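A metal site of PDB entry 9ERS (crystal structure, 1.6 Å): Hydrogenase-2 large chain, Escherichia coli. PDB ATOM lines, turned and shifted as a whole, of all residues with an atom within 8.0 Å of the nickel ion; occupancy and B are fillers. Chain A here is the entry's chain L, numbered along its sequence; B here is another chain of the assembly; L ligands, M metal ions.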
ATOM      1  N   GLU A  14      -1.677 -16.584  11.938  1.00  0.00           N
ATOM      2  CA  GLU A  14      -1.833 -15.367  12.721  1.00  0.00           C
ATOM      3  C   GLU A  14      -2.433 -15.756  14.061  1.00  0.00           C
ATOM      4  O   GLU A  14      -3.480 -16.426  14.128  1.00  0.00           O
ATOM      5  CB  GLU A  14      -2.729 -14.357  11.993  1.00  0.00           C
ATOM      6  CG  GLU A  14      -2.736 -12.984  12.646  1.00  0.00           C
ATOM      7  CD  GLU A  14      -3.323 -12.919  14.055  1.00  0.00           C
ATOM      8  OE1 GLU A  14      -4.276 -13.682  14.303  1.00  0.00           O
ATOM      9  OE2 GLU A  14      -2.821 -12.130  14.914  1.00  0.00           O
ATOM     10  N   GLY A  15      -1.819 -15.290  15.135  1.00  0.00           N
ATOM     11  CA  GLY A  15      -2.441 -15.328  16.446  1.00  0.00           C
ATOM     12  C   GLY A  15      -2.123 -16.607  17.227  1.00  0.00           C
ATOM     13  O   GLY A  15      -1.206 -17.374  16.903  1.00  0.00           O
ATOM     14  N   GLN A  58     -10.459  -2.114  12.668  1.00  0.00           N
ATOM     15  CA  GLN A  58      -9.449  -2.584  11.717  1.00  0.00           C
ATOM     16  C   GLN A  58      -8.369  -3.352  12.478  1.00  0.00           C
ATOM     17  O   GLN A  58      -7.801  -4.301  11.945  1.00  0.00           O
ATOM     18  CB  GLN A  58      -8.771  -1.461  10.942  1.00  0.00           C
ATOM     19  CG  GLN A  58      -7.875  -1.991   9.819  1.00  0.00           C
ATOM     20  CD  GLN A  58      -7.376  -0.996   8.800  1.00  0.00           C
ATOM     21  OE1 GLN A  58      -7.004  -1.369   7.692  1.00  0.00           O
ATOM     22  NE2 GLN A  58      -7.305   0.271   9.185  1.00  0.00           N
ATOM     23  N   ILE A  60      -8.563  -5.454  14.718  1.00  0.00           N
ATOM     24  CA  ILE A  60      -8.830  -6.844  14.999  1.00  0.00           C
ATOM     25  C   ILE A  60      -7.690  -7.679  14.417  1.00  0.00           C
ATOM     26  O   ILE A  60      -7.234  -8.643  15.052  1.00  0.00           O
ATOM     27  CB  ILE A  60     -10.210  -7.257  14.469  1.00  0.00           C
ATOM     28  CG1 ILE A  60     -11.306  -6.725  15.408  1.00  0.00           C
ATOM     29  CG2 ILE A  60     -10.303  -8.766  14.268  1.00  0.00           C
ATOM     30  CD1 ILE A  60     -12.706  -6.921  14.880  1.00  0.00           C
ATOM     31  N   CYS A  61      -7.198  -7.302  13.220  1.00  0.00           N
ATOM     32  CA  CYS A  61      -6.148  -8.086  12.580  1.00  0.00           C
ATOM     33  C   CYS A  61      -5.300  -7.232  11.647  1.00  0.00           C
ATOM     34  O   CYS A  61      -5.828  -6.448  10.855  1.00  0.00           O
ATOM     35  CB  CYS A  61      -6.773  -9.227  11.778  1.00  0.00           C
ATOM     36  SG  CYS A  61      -5.605 -10.481  11.196  1.00  0.00           S
ATOM     37  N   GLY A  62      -3.981  -7.464  11.699  1.00  0.00           N
ATOM     38  CA  GLY A  62      -3.030  -6.784  10.843  1.00  0.00           C
ATOM     39  C   GLY A  62      -2.526  -7.663   9.702  1.00  0.00           C
ATOM     40  O   GLY A  62      -1.835  -7.171   8.819  1.00  0.00           O
ATOM     41  N   VAL A  63      -2.886  -8.964   9.731  1.00  0.00           N
ATOM     42  CA  VAL A  63      -2.616  -9.832   8.603  1.00  0.00           C
ATOM     43  C   VAL A  63      -3.696  -9.555   7.551  1.00  0.00           C
ATOM     44  O   VAL A  63      -3.363  -9.142   6.453  1.00  0.00           O
ATOM     45  CB  VAL A  63      -2.572 -11.327   9.006  1.00  0.00           C
ATOM     46  CG1 VAL A  63      -2.489 -12.226   7.790  1.00  0.00           C
ATOM     47  CG2 VAL A  63      -1.421 -11.594   9.931  1.00  0.00           C
ATOM     48  N   CYS A  64      -4.978  -9.737   7.905  1.00  0.00           N
ATOM     49  CA  CYS A  64      -6.087  -9.328   7.057  1.00  0.00           C
ATOM     50  C   CYS A  64      -6.451  -7.877   7.392  1.00  0.00           C
ATOM     51  O   CYS A  64      -7.607  -7.532   7.654  1.00  0.00           O
ATOM     52  CB  CYS A  64      -7.294 -10.258   7.173  1.00  0.00           C
ATOM     53  SG  CYS A  64      -8.054 -10.306   8.818  1.00  0.00           S
ATOM     54  N   THR A  65      -5.420  -7.019   7.336  1.00  0.00           N
ATOM     55  CA  THR A  65      -5.620  -5.585   7.316  1.00  0.00           C
ATOM     56  C   THR A  65      -6.503  -5.228   6.129  1.00  0.00           C
ATOM     57  O   THR A  65      -6.664  -6.012   5.184  1.00  0.00           O
ATOM     58  CB  THR A  65      -4.273  -4.861   7.390  1.00  0.00           C
ATOM     59  OG1 THR A  65      -4.575  -3.486   7.667  1.00  0.00           O
ATOM     60  CG2 THR A  65      -3.427  -4.957   6.133  1.00  0.00           C
ATOM     61  N   THR A  67      -9.631  -5.493   5.892  1.00  0.00           N
ATOM     62  CA  THR A  67     -10.909  -6.199   5.795  1.00  0.00           C
ATOM     63  C   THR A  67     -11.928  -5.722   6.826  1.00  0.00           C
ATOM     64  O   THR A  67     -13.093  -5.500   6.500  1.00  0.00           O
ATOM     65  CB  THR A  67     -10.721  -7.715   5.855  1.00  0.00           C
ATOM     66  OG1 THR A  67     -10.204  -8.050   7.149  1.00  0.00           O
ATOM     67  CG2 THR A  67      -9.819  -8.224   4.743  1.00  0.00           C
ATOM     68  N   HIS A  68     -11.522  -5.567   8.073  1.00  0.00           N
ATOM     69  CA  HIS A  68     -12.423  -5.118   9.143  1.00  0.00           C
ATOM     70  C   HIS A  68     -12.752  -3.631   9.001  1.00  0.00           C
ATOM     71  O   HIS A  68     -13.852  -3.217   9.346  1.00  0.00           O
ATOM     72  CB  HIS A  68     -11.803  -5.441  10.502  1.00  0.00           C
ATOM     73  CG  HIS A  68     -11.747  -6.912  10.759  1.00  0.00           C
ATOM     74  ND1 HIS A  68     -12.843  -7.678  11.114  1.00  0.00           N
ATOM     75  CD2 HIS A  68     -10.685  -7.767  10.715  1.00  0.00           C
ATOM     76  CE1 HIS A  68     -12.468  -8.942  11.254  1.00  0.00           C
ATOM     77  NE2 HIS A  68     -11.158  -9.028  11.000  1.00  0.00           N
ATOM     78  N   HIS A  99      -4.617  -6.252  -1.470  1.00  0.00           N
ATOM     79  CA  HIS A  99      -4.351  -6.795  -0.149  1.00  0.00           C
ATOM     80  C   HIS A  99      -4.410  -8.327  -0.197  1.00  0.00           C
ATOM     81  O   HIS A  99      -3.508  -9.004   0.277  1.00  0.00           O
ATOM     82  CB  HIS A  99      -5.294  -6.260   0.937  1.00  0.00           C
ATOM     83  CG  HIS A  99      -5.088  -7.089   2.138  1.00  0.00           C
ATOM     84  ND1 HIS A  99      -4.014  -6.836   2.974  1.00  0.00           N
ATOM     85  CD2 HIS A  99      -5.613  -8.259   2.520  1.00  0.00           C
ATOM     86  CE1 HIS A  99      -3.959  -7.807   3.874  1.00  0.00           C
ATOM     87  NE2 HIS A  99      -4.930  -8.687   3.615  1.00  0.00           N
ATOM     88  N   ASP A 103      -1.803 -11.318   0.778  1.00  0.00           N
ATOM     89  CA  ASP A 103      -2.200 -12.188   1.860  1.00  0.00           C
ATOM     90  C   ASP A 103      -2.033 -13.648   1.418  1.00  0.00           C
ATOM     91  O   ASP A 103      -1.350 -14.420   2.074  1.00  0.00           O
ATOM     92  CB  ASP A 103      -3.641 -11.816   2.271  1.00  0.00           C
ATOM     93  CG  ASP A 103      -4.019 -12.261   3.660  1.00  0.00           C
ATOM     94  OD1 ASP A 103      -3.505 -13.318   4.089  1.00  0.00           O
ATOM     95  OD2 ASP A 103      -4.834 -11.566   4.292  1.00  0.00           O
ATOM     96  N   ALA A 477     -13.579 -11.904   2.584  1.00  0.00           N
ATOM     97  CA  ALA A 477     -12.217 -11.672   3.034  1.00  0.00           C
ATOM     98  C   ALA A 477     -11.337 -12.803   2.548  1.00  0.00           C
ATOM     99  O   ALA A 477     -11.848 -13.822   2.093  1.00  0.00           O
ATOM    100  CB  ALA A 477     -12.143 -11.541   4.537  1.00  0.00           C
ATOM    101  N   PRO A 478      -9.994 -12.683   2.675  1.00  0.00           N
ATOM    102  CA  PRO A 478      -9.091 -13.754   2.267  1.00  0.00           C
ATOM    103  C   PRO A 478      -9.394 -15.125   2.881  1.00  0.00           C
ATOM    104  O   PRO A 478      -9.198 -16.138   2.218  1.00  0.00           O
ATOM    105  CB  PRO A 478      -7.716 -13.238   2.715  1.00  0.00           C
ATOM    106  CG  PRO A 478      -7.858 -11.725   2.609  1.00  0.00           C
ATOM    107  CD  PRO A 478      -9.272 -11.453   3.074  1.00  0.00           C
ATOM    108  N   ARG A 479      -9.901 -15.146   4.123  1.00  0.00           N
ATOM    109  CA  ARG A 479     -10.198 -16.398   4.810  1.00  0.00           C
ATOM    110  C   ARG A 479     -11.691 -16.709   4.844  1.00  0.00           C
ATOM    111  O   ARG A 479     -12.074 -17.737   5.387  1.00  0.00           O
ATOM    112  CB  ARG A 479      -9.659 -16.321   6.239  1.00  0.00           C
ATOM    113  CG  ARG A 479      -8.137 -16.245   6.273  1.00  0.00           C
ATOM    114  CD  ARG A 479      -7.574 -15.652   7.546  1.00  0.00           C
ATOM    115  NE  ARG A 479      -6.124 -15.594   7.389  1.00  0.00           N
ATOM    116  CZ  ARG A 479      -5.459 -14.680   6.657  1.00  0.00           C
ATOM    117  NH1 ARG A 479      -6.068 -13.599   6.190  1.00  0.00           N
ATOM    118  NH2 ARG A 479      -4.149 -14.821   6.448  1.00  0.00           N
ATOM    119  N   VAL A 500     -16.401 -13.525  12.198  1.00  0.00           N
ATOM    120  CA  VAL A 500     -15.235 -13.425  11.339  1.00  0.00           C
ATOM    121  C   VAL A 500     -14.982 -14.782  10.677  1.00  0.00           C
ATOM    122  O   VAL A 500     -15.328 -15.806  11.255  1.00  0.00           O
ATOM    123  CB  VAL A 500     -14.048 -12.907  12.188  1.00  0.00           C
ATOM    124  CG1 VAL A 500     -12.797 -12.622  11.370  1.00  0.00           C
ATOM    125  CG2 VAL A 500     -14.451 -11.686  12.983  1.00  0.00           C
ATOM    126  N   PRO A 501     -14.438 -14.886   9.438  1.00  0.00           N
ATOM    127  CA  PRO A 501     -14.330 -16.187   8.794  1.00  0.00           C
ATOM    128  C   PRO A 501     -13.657 -17.267   9.643  1.00  0.00           C
ATOM    129  O   PRO A 501     -14.159 -18.387   9.733  1.00  0.00           O
ATOM    130  CB  PRO A 501     -13.556 -15.905   7.492  1.00  0.00           C
ATOM    131  CG  PRO A 501     -13.104 -14.473   7.589  1.00  0.00           C
ATOM    132  CD  PRO A 501     -14.041 -13.790   8.550  1.00  0.00           C
ATOM    133  N   SER A 502     -12.539 -16.939  10.296  1.00  0.00           N
ATOM    134  CA  SER A 502     -11.889 -17.907  11.155  1.00  0.00           C
ATOM    135  C   SER A 502     -12.747 -18.285  12.357  1.00  0.00           C
ATOM    136  O   SER A 502     -12.488 -19.330  12.977  1.00  0.00           O
ATOM    137  CB  SER A 502     -10.524 -17.442  11.577  1.00  0.00           C
ATOM    138  OG  SER A 502      -9.625 -17.516  10.453  1.00  0.00           O
ATOM    139  N   ASP A 544      -5.785 -21.438   6.733  1.00  0.00           N
ATOM    140  CA  ASP A 544      -5.189 -20.113   6.909  1.00  0.00           C
ATOM    141  C   ASP A 544      -5.694 -19.488   8.206  1.00  0.00           C
ATOM    142  O   ASP A 544      -6.317 -18.417   8.208  1.00  0.00           O
ATOM    143  CB  ASP A 544      -5.476 -19.276   5.666  1.00  0.00           C
ATOM    144  CG  ASP A 544      -4.815 -17.927   5.575  1.00  0.00           C
ATOM    145  OD1 ASP A 544      -3.947 -17.601   6.443  1.00  0.00           O
ATOM    146  OD2 ASP A 544      -5.213 -17.204   4.651  1.00  0.00           O
ATOM    147  N   PRO A 545      -5.487 -20.133   9.376  1.00  0.00           N
ATOM    148  CA  PRO A 545      -6.056 -19.631  10.628  1.00  0.00           C
ATOM    149  C   PRO A 545      -5.573 -18.230  10.965  1.00  0.00           C
ATOM    150  O   PRO A 545      -4.394 -17.884  10.818  1.00  0.00           O
ATOM    151  CB  PRO A 545      -5.544 -20.611  11.688  1.00  0.00           C
ATOM    152  CG  PRO A 545      -5.248 -21.852  10.916  1.00  0.00           C
ATOM    153  CD  PRO A 545      -4.707 -21.375   9.597  1.00  0.00           C
ATOM    154  N   CYS A 546      -6.521 -17.422  11.419  1.00  0.00           N
ATOM    155  CA  CYS A 546      -6.219 -16.098  11.954  1.00  0.00           C
ATOM    156  C   CYS A 546      -7.001 -15.949  13.266  1.00  0.00           C
ATOM    157  O   CYS A 546      -8.220 -15.793  13.239  1.00  0.00           O
ATOM    158  CB  CYS A 546      -6.606 -15.047  10.920  1.00  0.00           C
ATOM    159  SG  CYS A 546      -6.095 -13.398  11.397  1.00  0.00           S
ATOM    160  N   MET A 547      -6.300 -16.049  14.391  1.00  0.00           N
ATOM    161  CA  MET A 547      -6.980 -16.187  15.685  1.00  0.00           C
ATOM    162  C   MET A 547      -7.274 -14.826  16.316  1.00  0.00           C
ATOM    163  O   MET A 547      -8.197 -14.720  17.125  1.00  0.00           O
ATOM    164  CB  MET A 547      -6.177 -17.078  16.617  1.00  0.00           C
ATOM    165  CG  MET A 547      -5.948 -18.467  16.084  1.00  0.00           C
ATOM    166  SD  MET A 547      -7.380 -19.279  15.360  1.00  0.00           S
ATOM    167  CE  MET A 547      -8.393 -19.439  16.828  1.00  0.00           C
ATOM    168  N   ALA A 548      -6.523 -13.779  15.952  1.00  0.00           N
ATOM    169  CA  ALA A 548      -6.905 -12.430  16.317  1.00  0.00           C
ATOM    170  C   ALA A 548      -8.248 -12.134  15.670  1.00  0.00           C
ATOM    171  O   ALA A 548      -9.128 -11.560  16.291  1.00  0.00           O
ATOM    172  CB  ALA A 548      -5.834 -11.437  15.904  1.00  0.00           C
ATOM    173  N   CYS A 549      -8.409 -12.552  14.416  1.00  0.00           N
ATOM    174  CA  CYS A 549      -9.704 -12.544  13.720  1.00  0.00           C
ATOM    175  C   CYS A 549     -10.771 -13.391  14.412  1.00  0.00           C
ATOM    176  O   CYS A 549     -11.912 -12.953  14.598  1.00  0.00           O
ATOM    177  CB  CYS A 549      -9.512 -12.986  12.277  1.00  0.00           C
ATOM    178  SG  CYS A 549      -9.221 -11.581  11.180  1.00  0.00           S
ATOM    179  N   ALA A 550     -10.428 -14.648  14.712  1.00  0.00           N
ATOM    180  CA  ALA A 550     -11.421 -15.604  15.192  1.00  0.00           C
ATOM    181  C   ALA A 550     -12.066 -15.104  16.477  1.00  0.00           C
ATOM    182  O   ALA A 550     -13.266 -15.233  16.626  1.00  0.00           O
ATOM    183  CB  ALA A 550     -10.779 -16.960  15.366  1.00  0.00           C
ATOM    184  N   CYS B  21      -2.163  -7.919  16.926  1.00  0.00           N
ATOM    185  CA  CYS B  21      -2.970  -8.160  15.735  1.00  0.00           C
ATOM    186  C   CYS B  21      -2.077  -8.683  14.601  1.00  0.00           C
ATOM    187  O   CYS B  21      -2.607  -9.073  13.558  1.00  0.00           O
ATOM    188  CB  CYS B  21      -3.687  -6.889  15.317  1.00  0.00           C
ATOM    189  SG  CYS B  21      -2.659  -5.708  14.400  1.00  0.00           S
ATOM    190  N   THR B  22      -0.742  -8.671  14.810  1.00  0.00           N
ATOM    191  CA  THR B  22       0.295  -9.151  13.889  1.00  0.00           C
ATOM    192  C   THR B  22       0.685  -8.077  12.857  1.00  0.00           C
ATOM    193  O   THR B  22       1.622  -8.254  12.088  1.00  0.00           O
ATOM    194  CB  THR B  22      -0.063 -10.490  13.227  1.00  0.00           C
ATOM    195  OG1 THR B  22      -0.465 -11.368  14.280  1.00  0.00           O
ATOM    196  CG2 THR B  22       1.109 -11.145  12.523  1.00  0.00           C
HETATM  197 FE1  LIG L   1      -9.305 -12.206   8.981  1.00  0.00          FE
HETATM  198  C1  LIG L   1      -9.929 -13.898   9.386  1.00  0.00           C
HETATM  199  N1  LIG L   1     -10.332 -14.939   9.686  1.00  0.00           N
HETATM  200  C2  LIG L   1      -9.212 -12.621   7.206  1.00  0.00           C
HETATM  201  N2  LIG L   1      -9.100 -12.937   6.101  1.00  0.00           N
HETATM  202  C3  LIG L   1     -10.928 -11.539   8.617  1.00  0.00           C
HETATM  203  O1  LIG L   1     -11.939 -11.113   8.343  1.00  0.00           O
HETATM  204 NI    NI M   1      -7.044 -11.839  10.202  1.00  0.00          NI
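The nearest printed residue that does not touch the nickel ion is Arg 479 (4.5 Å).
N1 of the ligand sits at hydrogen-bond distance from N of Ser 502 (3.0 Å).
NH1 of Arg 479 sits at hydrogen-bond distance from N2 of the ligand (3.1 Å).
An iron atom (FE1) of the ligand is bound by the side-chain sulfur (SG) of Cys 549 (2.3 Å).
The side-chain hydroxyl (OG) of Ser 502 lies within hydrogen-bond range of a nitrogen (N1) of the ligand, at 2.8 Å.
N of Arg 479 is in hydrogen-bond range of N2 of the ligand.
The side-chain sulfur (SG) of Cys 64 binds an iron atom (FE1) of the ligand, 2.3 Å away.
A ring nitrogen (NE2) of His 68 lies within hydrogen-bond range of an oxygen (O1) of the ligand, 3.5 Å away.
SG of Cys 546 binds the nickel ion, at 2.2 Å.
The side-chain sulfur (SG) of Cys 61 is bound to the nickel ion, 2.2 Å away.
The side-chain sulfur (SG) of Cys 64 is bound to the nickel ion.
SG of Cys 549 is bound to the nickel ion, at 2.4 Å.
The backbone NH (N) of Cys 546 is in hydrogen-bond range of the side-chain hydroxyl (OG) of Ser 502.
SG of Cys 549 lies close to NE2 of His 68 (3.2 Å).
O of Cys 64 lies within hydrogen-bond range of OG1 of Thr 67 (2.7 Å).
OE1 of Glu 14 lies close to SG of Cys 546 (3.4 Å).
The side-chain sulfur (SG) of Cys 61 lies close to the backbone NH (N) of Val 63.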
